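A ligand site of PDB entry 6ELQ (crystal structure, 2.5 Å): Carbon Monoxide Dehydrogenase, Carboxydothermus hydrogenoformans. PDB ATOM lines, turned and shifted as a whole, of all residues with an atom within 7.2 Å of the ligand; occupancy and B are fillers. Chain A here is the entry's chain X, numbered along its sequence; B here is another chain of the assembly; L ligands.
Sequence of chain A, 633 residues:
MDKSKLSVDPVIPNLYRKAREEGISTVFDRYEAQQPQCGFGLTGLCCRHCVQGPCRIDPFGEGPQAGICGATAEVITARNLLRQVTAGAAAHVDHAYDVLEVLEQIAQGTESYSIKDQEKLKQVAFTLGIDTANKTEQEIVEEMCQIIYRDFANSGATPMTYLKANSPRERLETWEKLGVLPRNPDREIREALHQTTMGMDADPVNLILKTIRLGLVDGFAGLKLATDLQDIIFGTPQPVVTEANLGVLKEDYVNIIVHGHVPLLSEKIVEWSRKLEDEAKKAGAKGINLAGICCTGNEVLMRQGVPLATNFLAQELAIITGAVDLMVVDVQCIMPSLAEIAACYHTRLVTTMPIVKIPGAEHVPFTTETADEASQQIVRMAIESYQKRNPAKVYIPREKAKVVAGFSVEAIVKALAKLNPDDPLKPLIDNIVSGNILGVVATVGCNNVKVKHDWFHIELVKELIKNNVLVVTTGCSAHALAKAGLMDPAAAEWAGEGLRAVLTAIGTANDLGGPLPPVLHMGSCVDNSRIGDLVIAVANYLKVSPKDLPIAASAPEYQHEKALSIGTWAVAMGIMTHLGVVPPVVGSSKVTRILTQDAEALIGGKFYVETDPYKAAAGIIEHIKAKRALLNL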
ATOM      1  N   CYS A  46     -21.909  -1.576  19.310  1.00  0.00           N
ATOM      2  CA  CYS A  46     -21.831  -0.543  20.330  1.00  0.00           C
ATOM      3  C   CYS A  46     -22.771  -0.933  21.460  1.00  0.00           C
ATOM      4  O   CYS A  46     -23.877  -1.420  21.204  1.00  0.00           O
ATOM      5  CB  CYS A  46     -22.190   0.838  19.791  1.00  0.00           C
ATOM      6  SG  CYS A  46     -22.347   2.084  21.089  1.00  0.00           S
ATOM      7  N   CYS A  47     -22.326  -0.732  22.695  1.00  0.00           N
ATOM      8  CA  CYS A  47     -23.108  -1.150  23.852  1.00  0.00           C
ATOM      9  C   CYS A  47     -23.066  -0.063  24.920  1.00  0.00           C
ATOM     10  O   CYS A  47     -21.999   0.429  25.276  1.00  0.00           O
ATOM     11  CB  CYS A  47     -22.585  -2.475  24.427  1.00  0.00           C
ATOM     12  SG  CYS A  47     -23.512  -3.060  25.869  1.00  0.00           S
ATOM     13  N   ARG A  48     -24.252   0.285  25.433  1.00  0.00           N
ATOM     14  CA  ARG A  48     -24.392   1.253  26.508  1.00  0.00           C
ATOM     15  C   ARG A  48     -25.233   0.699  27.649  1.00  0.00           C
ATOM     16  O   ARG A  48     -25.841   1.470  28.399  1.00  0.00           O
ATOM     17  CB  ARG A  48     -25.006   2.558  25.980  1.00  0.00           C
ATOM     18  CG  ARG A  48     -24.193   3.240  24.889  1.00  0.00           C
ATOM     19  CD  ARG A  48     -24.960   4.411  24.302  1.00  0.00           C
ATOM     20  NE  ARG A  48     -25.496   5.269  25.354  1.00  0.00           N
ATOM     21  CZ  ARG A  48     -26.524   6.098  25.190  1.00  0.00           C
ATOM     22  NH1 ARG A  48     -27.144   6.162  24.025  1.00  0.00           N
ATOM     23  NH2 ARG A  48     -26.941   6.843  26.202  1.00  0.00           N
ATOM     24  N   HIS A  49     -25.281  -0.624  27.792  1.00  0.00           N
ATOM     25  CA  HIS A  49     -26.118  -1.265  28.810  1.00  0.00           C
ATOM     26  C   HIS A  49     -25.583  -1.102  30.220  1.00  0.00           C
ATOM     27  O   HIS A  49     -26.210  -1.606  31.154  1.00  0.00           O
ATOM     28  CB  HIS A  49     -26.288  -2.754  28.478  1.00  0.00           C
ATOM     29  CG  HIS A  49     -27.208  -3.010  27.325  1.00  0.00           C
ATOM     30  ND1 HIS A  49     -27.814  -4.234  27.105  1.00  0.00           N
ATOM     31  CD2 HIS A  49     -27.635  -2.194  26.331  1.00  0.00           C
ATOM     32  CE1 HIS A  49     -28.563  -4.156  26.026  1.00  0.00           C
ATOM     33  NE2 HIS A  49     -28.475  -2.942  25.536  1.00  0.00           N
ATOM     34  N   CYS A  50     -24.447  -0.433  30.396  1.00  0.00           N
ATOM     35  CA  CYS A  50     -23.995  -0.025  31.719  1.00  0.00           C
ATOM     36  C   CYS A  50     -23.275   1.299  31.589  1.00  0.00           C
ATOM     37  O   CYS A  50     -22.824   1.678  30.503  1.00  0.00           O
ATOM     38  CB  CYS A  50     -23.093  -1.086  32.369  1.00  0.00           C
ATOM     39  SG  CYS A  50     -21.361  -0.974  31.891  1.00  0.00           S
ATOM     40  N   VAL A  51     -23.162   2.009  32.715  1.00  0.00           N
ATOM     41  CA  VAL A  51     -22.555   3.344  32.727  1.00  0.00           C
ATOM     42  C   VAL A  51     -21.040   3.310  32.628  1.00  0.00           C
ATOM     43  O   VAL A  51     -20.399   4.364  32.666  1.00  0.00           O
ATOM     44  CB  VAL A  51     -23.032   4.087  33.987  1.00  0.00           C
ATOM     45  CG1 VAL A  51     -22.850   5.593  33.844  1.00  0.00           C
ATOM     46  CG2 VAL A  51     -24.491   3.768  34.274  1.00  0.00           C
ATOM     47  N   GLN A  52     -20.431   2.128  32.487  1.00  0.00           N
ATOM     48  CA  GLN A  52     -19.020   2.091  32.132  1.00  0.00           C
ATOM     49  C   GLN A  52     -18.807   2.399  30.659  1.00  0.00           C
ATOM     50  O   GLN A  52     -17.723   2.859  30.271  1.00  0.00           O
ATOM     51  CB  GLN A  52     -18.399   0.729  32.461  1.00  0.00           C
ATOM     52  CG  GLN A  52     -18.414   0.378  33.944  1.00  0.00           C
ATOM     53  CD  GLN A  52     -17.472  -0.772  34.272  1.00  0.00           C
ATOM     54  OE1 GLN A  52     -16.327  -0.550  34.676  1.00  0.00           O
ATOM     55  NE2 GLN A  52     -17.955  -2.002  34.109  1.00  0.00           N
ATOM     56  N   GLY A  53     -19.816   2.157  29.820  1.00  0.00           N
ATOM     57  CA  GLY A  53     -19.722   2.399  28.410  1.00  0.00           C
ATOM     58  C   GLY A  53     -19.797   3.866  28.047  1.00  0.00           C
ATOM     59  O   GLY A  53     -19.753   4.745  28.915  1.00  0.00           O
ATOM     60  N   PRO A  54     -19.953   4.162  26.742  1.00  0.00           N
ATOM     61  CA  PRO A  54     -20.146   3.209  25.651  1.00  0.00           C
ATOM     62  C   PRO A  54     -18.907   2.380  25.306  1.00  0.00           C
ATOM     63  O   PRO A  54     -17.780   2.874  25.413  1.00  0.00           O
ATOM     64  CB  PRO A  54     -20.535   4.097  24.467  1.00  0.00           C
ATOM     65  CG  PRO A  54     -20.826   5.441  25.042  1.00  0.00           C
ATOM     66  CD  PRO A  54     -19.984   5.547  26.263  1.00  0.00           C
ATOM     67  N   CYS A  55     -19.126   1.141  24.888  1.00  0.00           N
ATOM     68  CA  CYS A  55     -18.072   0.256  24.392  1.00  0.00           C
ATOM     69  C   CYS A  55     -18.379  -0.091  22.949  1.00  0.00           C
ATOM     70  O   CYS A  55     -19.529  -0.383  22.601  1.00  0.00           O
ATOM     71  CB  CYS A  55     -17.974  -1.023  25.217  1.00  0.00           C
ATOM     72  SG  CYS A  55     -17.976  -0.799  26.993  1.00  0.00           S
ATOM     73  N   ARG A  56     -17.361  -0.063  22.099  1.00  0.00           N
ATOM     74  CA  ARG A  56     -17.520  -0.425  20.698  1.00  0.00           C
ATOM     75  C   ARG A  56     -16.454  -1.438  20.316  1.00  0.00           C
ATOM     76  O   ARG A  56     -15.416  -1.559  20.966  1.00  0.00           O
ATOM     77  CB  ARG A  56     -17.474   0.801  19.783  1.00  0.00           C
ATOM     78  CG  ARG A  56     -16.465   1.854  20.165  1.00  0.00           C
ATOM     79  CD  ARG A  56     -16.712   3.155  19.419  1.00  0.00           C
ATOM     80  NE  ARG A  56     -15.859   4.230  19.902  1.00  0.00           N
ATOM     81  CZ  ARG A  56     -15.919   5.490  19.473  1.00  0.00           C
ATOM     82  NH1 ARG A  56     -15.090   6.398  19.980  1.00  0.00           N
ATOM     83  NH2 ARG A  56     -16.813   5.843  18.559  1.00  0.00           N
ATOM     84  N   ALA A  66     -13.541  -6.485  22.529  1.00  0.00           N
ATOM     85  CA  ALA A  66     -14.473  -6.762  23.608  1.00  0.00           C
ATOM     86  C   ALA A  66     -14.794  -5.467  24.334  1.00  0.00           C
ATOM     87  O   ALA A  66     -14.031  -4.497  24.270  1.00  0.00           O
ATOM     88  CB  ALA A  66     -13.910  -7.801  24.592  1.00  0.00           C
ATOM     89  N   GLY A  67     -15.949  -5.456  24.994  1.00  0.00           N
ATOM     90  CA  GLY A  67     -16.317  -4.351  25.841  1.00  0.00           C
ATOM     91  C   GLY A  67     -15.534  -4.371  27.140  1.00  0.00           C
ATOM     92  O   GLY A  67     -14.717  -5.253  27.418  1.00  0.00           O
ATOM     93  N   ILE A  68     -15.791  -3.345  27.971  1.00  0.00           N
ATOM     94  CA  ILE A  68     -15.073  -3.212  29.237  1.00  0.00           C
ATOM     95  C   ILE A  68     -15.363  -4.396  30.141  1.00  0.00           C
ATOM     96  O   ILE A  68     -14.475  -4.888  30.855  1.00  0.00           O
ATOM     97  CB  ILE A  68     -15.432  -1.871  29.903  1.00  0.00           C
ATOM     98  CG1 ILE A  68     -15.023  -0.715  28.990  1.00  0.00           C
ATOM     99  CG2 ILE A  68     -14.768  -1.746  31.260  1.00  0.00           C
ATOM    100  CD1 ILE A  68     -15.390   0.655  29.532  1.00  0.00           C
ATOM    101  N   CYS A  69     -16.600  -4.887  30.126  1.00  0.00           N
ATOM    102  CA  CYS A  69     -16.966  -6.058  30.917  1.00  0.00           C
ATOM    103  C   CYS A  69     -16.448  -7.355  30.314  1.00  0.00           C
ATOM    104  O   CYS A  69     -16.432  -8.384  30.996  1.00  0.00           O
ATOM    105  CB  CYS A  69     -18.482  -6.139  31.073  1.00  0.00           C
ATOM    106  SG  CYS A  69     -19.359  -6.456  29.522  1.00  0.00           S
ATOM    107  N   GLY A  70     -16.035  -7.334  29.046  1.00  0.00           N
ATOM    108  CA  GLY A  70     -15.579  -8.516  28.341  1.00  0.00           C
ATOM    109  C   GLY A  70     -16.534  -9.043  27.299  1.00  0.00           C
ATOM    110  O   GLY A  70     -16.258 -10.082  26.709  1.00  0.00           O
ATOM    111  N   ALA A  71     -17.655  -8.351  27.062  1.00  0.00           N
ATOM    112  CA  ALA A  71     -18.621  -8.801  26.057  1.00  0.00           C
ATOM    113  C   ALA A  71     -18.033  -8.666  24.654  1.00  0.00           C
ATOM    114  O   ALA A  71     -17.522  -7.606  24.286  1.00  0.00           O
ATOM    115  CB  ALA A  71     -19.908  -7.990  26.173  1.00  0.00           C
ATOM    116  N   THR A  72     -18.108  -9.751  23.884  1.00  0.00           N
ATOM    117  CA  THR A  72     -17.597  -9.761  22.521  1.00  0.00           C
ATOM    118  C   THR A  72     -18.723  -9.368  21.553  1.00  0.00           C
ATOM    119  O   THR A  72     -19.818  -8.980  21.957  1.00  0.00           O
ATOM    120  CB  THR A  72     -16.997 -11.126  22.189  1.00  0.00           C
ATOM    121  OG1 THR A  72     -17.990 -12.139  22.359  1.00  0.00           O
ATOM    122  CG2 THR A  72     -15.815 -11.417  23.098  1.00  0.00           C
ATOM    123  N   ILE A  76     -22.663  -8.708  22.455  1.00  0.00           N
ATOM    124  CA  ILE A  76     -23.207  -7.350  22.347  1.00  0.00           C
ATOM    125  C   ILE A  76     -24.357  -7.316  21.359  1.00  0.00           C
ATOM    126  O   ILE A  76     -25.427  -6.751  21.641  1.00  0.00           O
ATOM    127  CB  ILE A  76     -22.096  -6.364  21.961  1.00  0.00           C
ATOM    128  CG1 ILE A  76     -21.087  -6.223  23.102  1.00  0.00           C
ATOM    129  CG2 ILE A  76     -22.687  -5.020  21.580  1.00  0.00           C
ATOM    130  CD1 ILE A  76     -19.964  -5.253  22.814  1.00  0.00           C
ATOM    131  N   ARG A  79     -27.375  -9.630  22.677  1.00  0.00           N
ATOM    132  CA  ARG A  79     -28.007  -9.005  23.830  1.00  0.00           C
ATOM    133  C   ARG A  79     -28.871  -7.822  23.400  1.00  0.00           C
ATOM    134  O   ARG A  79     -29.977  -7.630  23.918  1.00  0.00           O
ATOM    135  CB  ARG A  79     -26.955  -8.572  24.848  1.00  0.00           C
ATOM    136  CG  ARG A  79     -27.465  -7.677  25.954  1.00  0.00           C
ATOM    137  CD  ARG A  79     -26.377  -7.448  26.992  1.00  0.00           C
ATOM    138  NE  ARG A  79     -25.188  -6.835  26.408  1.00  0.00           N
ATOM    139  CZ  ARG A  79     -23.973  -6.859  26.971  1.00  0.00           C
ATOM    140  NH1 ARG A  79     -22.947  -6.283  26.375  1.00  0.00           N
ATOM    141  NH2 ARG A  79     -23.803  -7.484  28.133  1.00  0.00           N
ATOM    142  N   THR A 196     -30.863  -8.960  29.760  1.00  0.00           N
ATOM    143  CA  THR A 196     -30.041  -8.102  28.917  1.00  0.00           C
ATOM    144  C   THR A 196     -29.248  -7.070  29.715  1.00  0.00           C
ATOM    145  O   THR A 196     -28.506  -6.292  29.110  1.00  0.00           O
ATOM    146  CB  THR A 196     -30.898  -7.398  27.857  1.00  0.00           C
ATOM    147  OG1 THR A 196     -31.797  -6.486  28.485  1.00  0.00           O
ATOM    148  CG2 THR A 196     -31.689  -8.408  27.055  1.00  0.00           C
ATOM    149  N   THR A 197     -29.401  -7.046  31.039  1.00  0.00           N
ATOM    150  CA  THR A 197     -28.600  -6.140  31.852  1.00  0.00           C
ATOM    151  C   THR A 197     -27.152  -6.611  31.896  1.00  0.00           C
ATOM    152  O   THR A 197     -26.804  -7.709  31.442  1.00  0.00           O
ATOM    153  CB  THR A 197     -29.182  -6.049  33.266  1.00  0.00           C
ATOM    154  OG1 THR A 197     -29.015  -7.297  33.939  1.00  0.00           O
ATOM    155  CG2 THR A 197     -30.651  -5.700  33.222  1.00  0.00           C
ATOM    156  N   MET A 198     -26.289  -5.769  32.453  1.00  0.00           N
ATOM    157  CA  MET A 198     -24.857  -6.040  32.441  1.00  0.00           C
ATOM    158  C   MET A 198     -24.536  -7.283  33.251  1.00  0.00           C
ATOM    159  O   MET A 198     -25.119  -7.535  34.307  1.00  0.00           O
ATOM    160  CB  MET A 198     -24.082  -4.830  32.996  1.00  0.00           C
ATOM    161  CG  MET A 198     -22.579  -5.033  33.071  1.00  0.00           C
ATOM    162  SD  MET A 198     -22.016  -5.817  34.603  1.00  0.00           S
ATOM    163  CE  MET A 198     -20.469  -6.539  34.065  1.00  0.00           C
ATOM    164  N   GLY A 199     -23.589  -8.076  32.743  1.00  0.00           N
ATOM    165  CA  GLY A 199     -23.088  -9.234  33.472  1.00  0.00           C
ATOM    166  C   GLY A 199     -24.070 -10.376  33.578  1.00  0.00           C
ATOM    167  O   GLY A 199     -24.114 -11.057  34.604  1.00  0.00           O
ATOM    168  N   GLN B  34     -10.710   1.283  24.944  1.00  0.00           N
ATOM    169  CA  GLN B  34     -11.906   1.996  24.523  1.00  0.00           C
ATOM    170  C   GLN B  34     -11.718   3.506  24.508  1.00  0.00           C
ATOM    171  O   GLN B  34     -12.491   4.205  23.840  1.00  0.00           O
ATOM    172  CB  GLN B  34     -13.080   1.655  25.443  1.00  0.00           C
ATOM    173  CG  GLN B  34     -13.551   0.215  25.349  1.00  0.00           C
ATOM    174  CD  GLN B  34     -14.338  -0.063  24.074  1.00  0.00           C
ATOM    175  OE1 GLN B  34     -14.892   0.853  23.460  1.00  0.00           O
ATOM    176  NE2 GLN B  34     -14.389  -1.322  23.676  1.00  0.00           N
ATOM    177  N   GLN B  37     -13.841   7.386  24.576  1.00  0.00           N
ATOM    178  CA  GLN B  37     -15.178   6.840  24.376  1.00  0.00           C
ATOM    179  C   GLN B  37     -16.076   7.861  23.672  1.00  0.00           C
ATOM    180  O   GLN B  37     -15.865   9.074  23.774  1.00  0.00           O
ATOM    181  CB  GLN B  37     -15.806   6.422  25.712  1.00  0.00           C
ATOM    182  CG  GLN B  37     -15.078   5.259  26.385  1.00  0.00           C
ATOM    183  CD  GLN B  37     -15.630   4.925  27.752  1.00  0.00           C
ATOM    184  OE1 GLN B  37     -15.305   5.568  28.744  1.00  0.00           O
ATOM    185  NE2 GLN B  37     -16.483   3.907  27.816  1.00  0.00           N
ATOM    186  N   PHE B 312     -16.721  -5.648  42.605  1.00  0.00           N
ATOM    187  CA  PHE B 312     -17.058  -5.888  41.203  1.00  0.00           C
ATOM    188  C   PHE B 312     -15.842  -5.754  40.295  1.00  0.00           C
ATOM    189  O   PHE B 312     -15.569  -6.633  39.466  1.00  0.00           O
ATOM    190  CB  PHE B 312     -18.164  -4.928  40.767  1.00  0.00           C
ATOM    191  CG  PHE B 312     -18.294  -4.787  39.281  1.00  0.00           C
ATOM    192  CD1 PHE B 312     -18.923  -5.765  38.533  1.00  0.00           C
ATOM    193  CD2 PHE B 312     -17.818  -3.658  38.628  1.00  0.00           C
ATOM    194  CE1 PHE B 312     -19.054  -5.637  37.159  1.00  0.00           C
ATOM    195  CE2 PHE B 312     -17.938  -3.525  37.262  1.00  0.00           C
ATOM    196  CZ  PHE B 312     -18.565  -4.515  36.520  1.00  0.00           C
ATOM    197  N   PRO B 336     -18.133 -11.555  31.538  1.00  0.00           N
ATOM    198  CA  PRO B 336     -17.944 -12.734  30.675  1.00  0.00           C
ATOM    199  C   PRO B 336     -16.480 -13.069  30.421  1.00  0.00           C
ATOM    200  O   PRO B 336     -16.189 -14.172  29.945  1.00  0.00           O
ATOM    201  CB  PRO B 336     -18.662 -12.348  29.374  1.00  0.00           C
ATOM    202  CG  PRO B 336     -18.689 -10.857  29.391  1.00  0.00           C
ATOM    203  CD  PRO B 336     -18.832 -10.467  30.828  1.00  0.00           C
ATOM    204  N   GLN B 559     -22.300   1.558  38.115  1.00  0.00           N
ATOM    205  CA  GLN B 559     -22.124   1.148  36.725  1.00  0.00           C
ATOM    206  C   GLN B 559     -23.379   0.452  36.189  1.00  0.00           C
ATOM    207  O   GLN B 559     -23.758   0.662  35.036  1.00  0.00           O
ATOM    208  CB  GLN B 559     -20.898   0.235  36.584  1.00  0.00           C
ATOM    209  CG  GLN B 559     -21.002  -1.108  37.301  1.00  0.00           C
ATOM    210  CD  GLN B 559     -21.566  -2.209  36.426  1.00  0.00           C
ATOM    211  OE1 GLN B 559     -21.529  -2.116  35.198  1.00  0.00           O
ATOM    212  NE2 GLN B 559     -22.093  -3.258  37.051  1.00  0.00           N
HETATM  213 FE1  LIG L   1     -20.147  -4.388  28.943  1.00  0.00          FE
HETATM  214 FE2  LIG L   1     -21.299  -2.210  30.010  1.00  0.00          FE
HETATM  215 FE3  LIG L   1     -19.708  -1.976  27.957  1.00  0.00          FE
HETATM  216 FE4  LIG L   1     -21.998  -3.091  27.636  1.00  0.00          FE
HETATM  217  S1  LIG L   1     -21.652  -0.993  28.300  1.00  0.00           S
HETATM  218  S2  LIG L   1     -20.119  -3.808  26.845  1.00  0.00           S
HETATM  219  S3  LIG L   1     -22.270  -4.110  29.512  1.00  0.00           S
HETATM  220  S4  LIG L   1     -19.155  -2.661  29.906  1.00  0.00           S
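N of Cys 69 lies close to S4 of the ligand, at 3.4 Å. S1 of the ligand sits close to N of Cys 50 (3.5 Å). NH1 of Arg 79 sits close to S2 of the ligand (3.8 Å). FE1 of the ligand is bound by SG of Cys 69 (2.3 Å). The side-chain sulfur (SG) of Cys 47 binds an iron atom (FE4) of the ligand (2.3 Å). The side-chain sulfur (SG) of Cys 50 is bound to an iron atom (FE2) of the ligand (2.3 Å). A sulfur (S1) of the ligand sits close to the backbone NH (N) of His 49, 3.7 Å away. The side-chain sulfur of Cys 55 is bound to an iron atom (FE3) of the ligand.
The backbone NH (N) of His 49 lies close to the side-chain sulfur (SG) of Cys 47. O of Cys 55 is in hydrogen-bond range of N of Cys 47 (2.8 Å). N of Gln 52 sits close to SG of Cys 50 (3.3 Å). A ring nitrogen (ND1) of His 49 is in hydrogen-bond range of the backbone carbonyl oxygen (O) of Thr 196, at 3.0 Å. The backbone NH (N) of Ala 71 lies close to the side-chain sulfur (SG) of Cys 69. SG of Cys 47 sits close to NH1 of Arg 79, 3.3 Å away. The side-chain sulfur (SG) of Cys 50 sits close to the side-chain amide oxygen (OE1) of Gln 559 of chain B (3.5 Å). SG of Cys 55 sits close to N of Ile 68 (3.5 Å).
Merely in contact with the ligand: Arg 48 (3.97 Å), Gly 53 (3.9 Å), Gly 67 (3.97 Å), Ile 68 (3.8 Å) and Met 198 (3.7 Å). Hydrophobic or aromatic side chains that line the ligand: Ile 68 and Met 198. The nearest printed residue that does not touch the ligand is Ala 71 (4.2 Å).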
